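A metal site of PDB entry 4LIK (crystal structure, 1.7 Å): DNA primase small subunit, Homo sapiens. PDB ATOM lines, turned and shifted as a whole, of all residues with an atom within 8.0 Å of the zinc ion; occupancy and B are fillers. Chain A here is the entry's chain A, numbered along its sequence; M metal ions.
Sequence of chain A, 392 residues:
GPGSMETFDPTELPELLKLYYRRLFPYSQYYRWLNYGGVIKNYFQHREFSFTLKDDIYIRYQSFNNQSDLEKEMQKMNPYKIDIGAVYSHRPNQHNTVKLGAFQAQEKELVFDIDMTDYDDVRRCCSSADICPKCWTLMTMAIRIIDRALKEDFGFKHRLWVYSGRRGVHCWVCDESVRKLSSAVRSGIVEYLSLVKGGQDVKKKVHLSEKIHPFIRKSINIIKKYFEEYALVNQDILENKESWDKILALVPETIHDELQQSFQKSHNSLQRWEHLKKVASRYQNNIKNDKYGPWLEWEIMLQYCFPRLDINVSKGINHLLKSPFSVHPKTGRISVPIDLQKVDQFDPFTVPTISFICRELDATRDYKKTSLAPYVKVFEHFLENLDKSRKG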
ATOM      1  N   MET A 116      29.635  22.613  36.696  1.00  0.00           N
ATOM      2  CA  MET A 116      29.625  21.301  36.063  1.00  0.00           C
ATOM      3  C   MET A 116      30.355  20.248  36.891  1.00  0.00           C
ATOM      4  O   MET A 116      30.032  19.071  36.806  1.00  0.00           O
ATOM      5  CB  MET A 116      30.281  21.385  34.688  1.00  0.00           C
ATOM      6  CG  MET A 116      30.003  20.176  33.817  1.00  0.00           C
ATOM      7  SD  MET A 116      28.302  20.214  33.219  1.00  0.00           S
ATOM      8  CE  MET A 116      28.439  21.518  31.988  1.00  0.00           C
ATOM      9  N   ARG A 123      27.641  12.406  34.192  1.00  0.00           N
ATOM     10  CA  ARG A 123      27.960  12.624  32.782  1.00  0.00           C
ATOM     11  C   ARG A 123      29.027  11.657  32.299  1.00  0.00           C
ATOM     12  O   ARG A 123      29.918  11.274  33.054  1.00  0.00           O
ATOM     13  CB  ARG A 123      28.302  14.094  32.465  1.00  0.00           C
ATOM     14  CG  ARG A 123      29.067  14.825  33.538  1.00  0.00           C
ATOM     15  CD  ARG A 123      29.537  16.202  33.048  1.00  0.00           C
ATOM     16  NE  ARG A 123      30.813  16.534  33.661  1.00  0.00           N
ATOM     17  CZ  ARG A 123      31.759  17.253  33.075  1.00  0.00           C
ATOM     18  NH1 ARG A 123      31.593  17.733  31.853  1.00  0.00           N
ATOM     19  NH2 ARG A 123      32.896  17.480  33.721  1.00  0.00           N
ATOM     20  N   ARG A 124      28.935  11.251  31.030  1.00  0.00           N
ATOM     21  CA  ARG A 124      29.785  10.213  30.469  1.00  0.00           C
ATOM     22  C   ARG A 124      30.610  10.772  29.325  1.00  0.00           C
ATOM     23  O   ARG A 124      31.418  10.053  28.728  1.00  0.00           O
ATOM     24  CB  ARG A 124      28.934   9.058  29.911  1.00  0.00           C
ATOM     25  CG  ARG A 124      27.997   8.386  30.886  1.00  0.00           C
ATOM     26  CD  ARG A 124      27.322   7.172  30.241  1.00  0.00           C
ATOM     27  NE  ARG A 124      28.307   6.232  29.692  1.00  0.00           N
ATOM     28  CZ  ARG A 124      28.369   5.873  28.412  1.00  0.00           C
ATOM     29  NH1 ARG A 124      27.494   6.350  27.539  1.00  0.00           N
ATOM     30  NH2 ARG A 124      29.302   5.019  28.009  1.00  0.00           N
ATOM     31  N   CYS A 125      30.386  12.036  29.000  1.00  0.00           N
ATOM     32  CA  CYS A 125      30.924  12.621  27.783  1.00  0.00           C
ATOM     33  C   CYS A 125      32.261  13.323  27.953  1.00  0.00           C
ATOM     34  O   CYS A 125      33.010  13.488  26.995  1.00  0.00           O
ATOM     35  CB  CYS A 125      29.912  13.600  27.192  1.00  0.00           C
ATOM     36  SG  CYS A 125      29.469  14.924  28.338  1.00  0.00           S
ATOM     37  N   CYS A 126      32.571  13.739  29.184  1.00  0.00           N
ATOM     38  CA  CYS A 126      33.795  14.504  29.447  1.00  0.00           C
ATOM     39  C   CYS A 126      34.566  13.988  30.651  1.00  0.00           C
ATOM     40  O   CYS A 126      34.022  13.301  31.507  1.00  0.00           O
ATOM     41  CB  CYS A 126      33.464  15.984  29.688  1.00  0.00           C
ATOM     42  SG  CYS A 126      32.922  16.901  28.231  1.00  0.00           S
ATOM     43  N   SER A 127      35.851  14.322  30.695  1.00  0.00           N
ATOM     44  CA  SER A 127      36.623  14.223  31.925  1.00  0.00           C
ATOM     45  C   SER A 127      36.131  15.339  32.831  1.00  0.00           C
ATOM     46  O   SER A 127      35.536  16.299  32.348  1.00  0.00           O
ATOM     47  CB  SER A 127      38.114  14.394  31.638  1.00  0.00           C
ATOM     48  OG  SER A 127      38.516  13.572  30.555  1.00  0.00           O
ATOM     49  N   ASP A 130      36.854  18.928  31.430  1.00  0.00           N
ATOM     50  CA  ASP A 130      36.301  19.488  30.195  1.00  0.00           C
ATOM     51  C   ASP A 130      34.793  19.724  30.284  1.00  0.00           C
ATOM     52  O   ASP A 130      34.139  19.252  31.210  1.00  0.00           O
ATOM     53  CB  ASP A 130      36.614  18.565  29.013  1.00  0.00           C
ATOM     54  CG  ASP A 130      38.098  18.360  28.806  1.00  0.00           C
ATOM     55  OD1 ASP A 130      38.888  19.129  29.395  1.00  0.00           O
ATOM     56  OD2 ASP A 130      38.468  17.427  28.049  1.00  0.00           O
ATOM     57  N   ILE A 131      34.273  20.485  29.326  1.00  0.00           N
ATOM     58  CA  ILE A 131      32.840  20.472  29.055  1.00  0.00           C
ATOM     59  C   ILE A 131      32.670  20.294  27.569  1.00  0.00           C
ATOM     60  O   ILE A 131      33.615  20.501  26.798  1.00  0.00           O
ATOM     61  CB  ILE A 131      32.132  21.760  29.532  1.00  0.00           C
ATOM     62  CG1 ILE A 131      32.735  23.003  28.879  1.00  0.00           C
ATOM     63  CG2 ILE A 131      32.219  21.880  31.048  1.00  0.00           C
ATOM     64  CD1 ILE A 131      31.916  24.272  29.120  1.00  0.00           C
ATOM     65  N   CYS A 132      31.489  19.875  27.138  1.00  0.00           N
ATOM     66  CA  CYS A 132      31.205  19.785  25.724  1.00  0.00           C
ATOM     67  C   CYS A 132      29.768  20.240  25.533  1.00  0.00           C
ATOM     68  O   CYS A 132      29.056  20.481  26.513  1.00  0.00           O
ATOM     69  CB  CYS A 132      31.390  18.367  25.220  1.00  0.00           C
ATOM     70  SG  CYS A 132      30.273  17.230  26.020  1.00  0.00           S
ATOM     71  N   PRO A 133      29.344  20.380  24.264  1.00  0.00           N
ATOM     72  CA  PRO A 133      27.990  20.802  23.900  1.00  0.00           C
ATOM     73  C   PRO A 133      26.935  19.816  24.384  1.00  0.00           C
ATOM     74  O   PRO A 133      25.758  20.155  24.522  1.00  0.00           O
ATOM     75  CB  PRO A 133      28.042  20.847  22.372  1.00  0.00           C
ATOM     76  CG  PRO A 133      29.485  21.133  22.056  1.00  0.00           C
ATOM     77  CD  PRO A 133      30.240  20.339  23.089  1.00  0.00           C
ATOM     78  N   LYS A 134      27.358  18.581  24.652  1.00  0.00           N
ATOM     79  CA  LYS A 134      26.461  17.561  25.175  1.00  0.00           C
ATOM     80  C   LYS A 134      26.096  17.801  26.637  1.00  0.00           C
ATOM     81  O   LYS A 134      24.920  17.781  27.003  1.00  0.00           O
ATOM     82  CB  LYS A 134      27.076  16.176  25.028  1.00  0.00           C
ATOM     83  CG  LYS A 134      27.320  15.781  23.590  1.00  0.00           C
ATOM     84  CD  LYS A 134      27.892  14.384  23.497  1.00  0.00           C
ATOM     85  CE  LYS A 134      27.892  13.895  22.060  1.00  0.00           C
ATOM     86  NZ  LYS A 134      28.927  12.852  21.829  1.00  0.00           N
ATOM     87  N   CYS A 135      27.101  18.031  27.479  1.00  0.00           N
ATOM     88  CA  CYS A 135      26.854  18.209  28.906  1.00  0.00           C
ATOM     89  C   CYS A 135      26.470  19.636  29.276  1.00  0.00           C
ATOM     90  O   CYS A 135      25.926  19.856  30.357  1.00  0.00           O
ATOM     91  CB  CYS A 135      28.039  17.708  29.765  1.00  0.00           C
ATOM     92  SG  CYS A 135      29.615  18.506  29.452  1.00  0.00           S
ATOM     93  N   TRP A 136      26.739  20.605  28.400  1.00  0.00           N
ATOM     94  CA  TRP A 136      26.312  21.960  28.707  1.00  0.00           C
ATOM     95  C   TRP A 136      24.797  22.027  28.919  1.00  0.00           C
ATOM     96  O   TRP A 136      24.297  22.899  29.647  1.00  0.00           O
ATOM     97  CB  TRP A 136      26.778  22.995  27.676  1.00  0.00           C
ATOM     98  CG  TRP A 136      26.394  24.386  28.121  1.00  0.00           C
ATOM     99  CD1 TRP A 136      25.336  25.131  27.676  1.00  0.00           C
ATOM    100  CD2 TRP A 136      27.029  25.159  29.139  1.00  0.00           C
ATOM    101  NE1 TRP A 136      25.287  26.326  28.345  1.00  0.00           N
ATOM    102  CE2 TRP A 136      26.326  26.374  29.255  1.00  0.00           C
ATOM    103  CE3 TRP A 136      28.139  24.950  29.967  1.00  0.00           C
ATOM    104  CZ2 TRP A 136      26.685  27.359  30.168  1.00  0.00           C
ATOM    105  CZ3 TRP A 136      28.502  25.948  30.862  1.00  0.00           C
ATOM    106  CH2 TRP A 136      27.777  27.132  30.957  1.00  0.00           C
ATOM    107  N   THR A 137      24.049  21.096  28.334  1.00  0.00           N
ATOM    108  CA  THR A 137      22.603  21.062  28.528  1.00  0.00           C
ATOM    109  C   THR A 137      22.234  20.991  30.010  1.00  0.00           C
ATOM    110  O   THR A 137      21.173  21.483  30.409  1.00  0.00           O
ATOM    111  CB  THR A 137      21.965  19.917  27.757  1.00  0.00           C
ATOM    112  OG1 THR A 137      22.247  20.067  26.357  1.00  0.00           O
ATOM    113  CG2 THR A 137      20.456  19.936  27.952  1.00  0.00           C
ATOM    114  N   LEU A 138      23.103  20.402  30.824  1.00  0.00           N
ATOM    115  CA  LEU A 138      22.886  20.398  32.261  1.00  0.00           C
ATOM    116  C   LEU A 138      22.734  21.829  32.820  1.00  0.00           C
ATOM    117  O   LEU A 138      21.896  22.068  33.720  1.00  0.00           O
ATOM    118  CB  LEU A 138      24.044  19.684  32.975  1.00  0.00           C
ATOM    119  CG  LEU A 138      24.065  18.182  32.784  1.00  0.00           C
ATOM    120  CD1 LEU A 138      25.363  17.620  33.337  1.00  0.00           C
ATOM    121  CD2 LEU A 138      22.872  17.577  33.508  1.00  0.00           C
ATOM    122  N   TYR A 230      18.940  14.584  25.667  1.00  0.00           N
ATOM    123  CA  TYR A 230      20.070  14.755  26.568  1.00  0.00           C
ATOM    124  C   TYR A 230      20.562  13.420  27.137  1.00  0.00           C
ATOM    125  O   TYR A 230      21.707  13.040  26.952  1.00  0.00           O
ATOM    126  CB  TYR A 230      19.734  15.700  27.722  1.00  0.00           C
ATOM    127  CG  TYR A 230      20.846  15.638  28.725  1.00  0.00           C
ATOM    128  CD1 TYR A 230      22.074  16.176  28.426  1.00  0.00           C
ATOM    129  CD2 TYR A 230      20.687  14.963  29.929  1.00  0.00           C
ATOM    130  CE1 TYR A 230      23.118  16.091  29.296  1.00  0.00           C
ATOM    131  CE2 TYR A 230      21.737  14.872  30.830  1.00  0.00           C
ATOM    132  CZ  TYR A 230      22.948  15.441  30.494  1.00  0.00           C
ATOM    133  OH  TYR A 230      24.017  15.368  31.339  1.00  0.00           O
ATOM    134  N   GLN A 235      23.930  11.497  26.266  1.00  0.00           N
ATOM    135  CA  GLN A 235      24.687  10.809  27.309  1.00  0.00           C
ATOM    136  C   GLN A 235      24.637   9.290  27.201  1.00  0.00           C
ATOM    137  O   GLN A 235      25.497   8.608  27.754  1.00  0.00           O
ATOM    138  CB  GLN A 235      24.192  11.228  28.697  1.00  0.00           C
ATOM    139  CG  GLN A 235      24.494  12.660  29.045  1.00  0.00           C
ATOM    140  CD  GLN A 235      25.973  12.969  28.979  1.00  0.00           C
ATOM    141  OE1 GLN A 235      26.804  12.156  29.375  1.00  0.00           O
ATOM    142  NE2 GLN A 235      26.302  14.150  28.472  1.00  0.00           N
ATOM    143  N   PHE A 349      31.439  28.125  24.383  1.00  0.00           N
ATOM    144  CA  PHE A 349      32.604  28.022  23.515  1.00  0.00           C
ATOM    145  C   PHE A 349      32.791  29.218  22.589  1.00  0.00           C
ATOM    146  O   PHE A 349      33.874  29.432  22.050  1.00  0.00           O
ATOM    147  CB  PHE A 349      32.537  26.712  22.736  1.00  0.00           C
ATOM    148  CG  PHE A 349      32.307  25.532  23.614  1.00  0.00           C
ATOM    149  CD1 PHE A 349      33.360  25.011  24.361  1.00  0.00           C
ATOM    150  CD2 PHE A 349      31.049  24.976  23.736  1.00  0.00           C
ATOM    151  CE1 PHE A 349      33.152  23.934  25.206  1.00  0.00           C
ATOM    152  CE2 PHE A 349      30.831  23.892  24.568  1.00  0.00           C
ATOM    153  CZ  PHE A 349      31.881  23.375  25.306  1.00  0.00           C
HETATM  154 ZN    ZN M   1      30.657  16.892  27.972  1.00  0.00          ZN
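SG of Cys 125 lies close to NE2 of Gln 235, 3.3 Å away.
The side-chain sulfur (SG) of Cys 132 sits close to the backbone NH (N) of Lys 134, at 3.5 Å.
SG of Cys 135 lies close to NH1 of Arg 123 (3.2 Å).
Ile 131 touches the zinc ion.
Within 4 Å of the zinc ion: Cys 125, Cys 126, Ile 131, Cys 132 and Cys 135.
The zinc ion is bound by SG of Cys 132 (2.0 Å), SG of Cys 126 (2.3 Å), SG of Cys 125 (2.3 Å) and SG of Cys 135 (2.4 Å).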
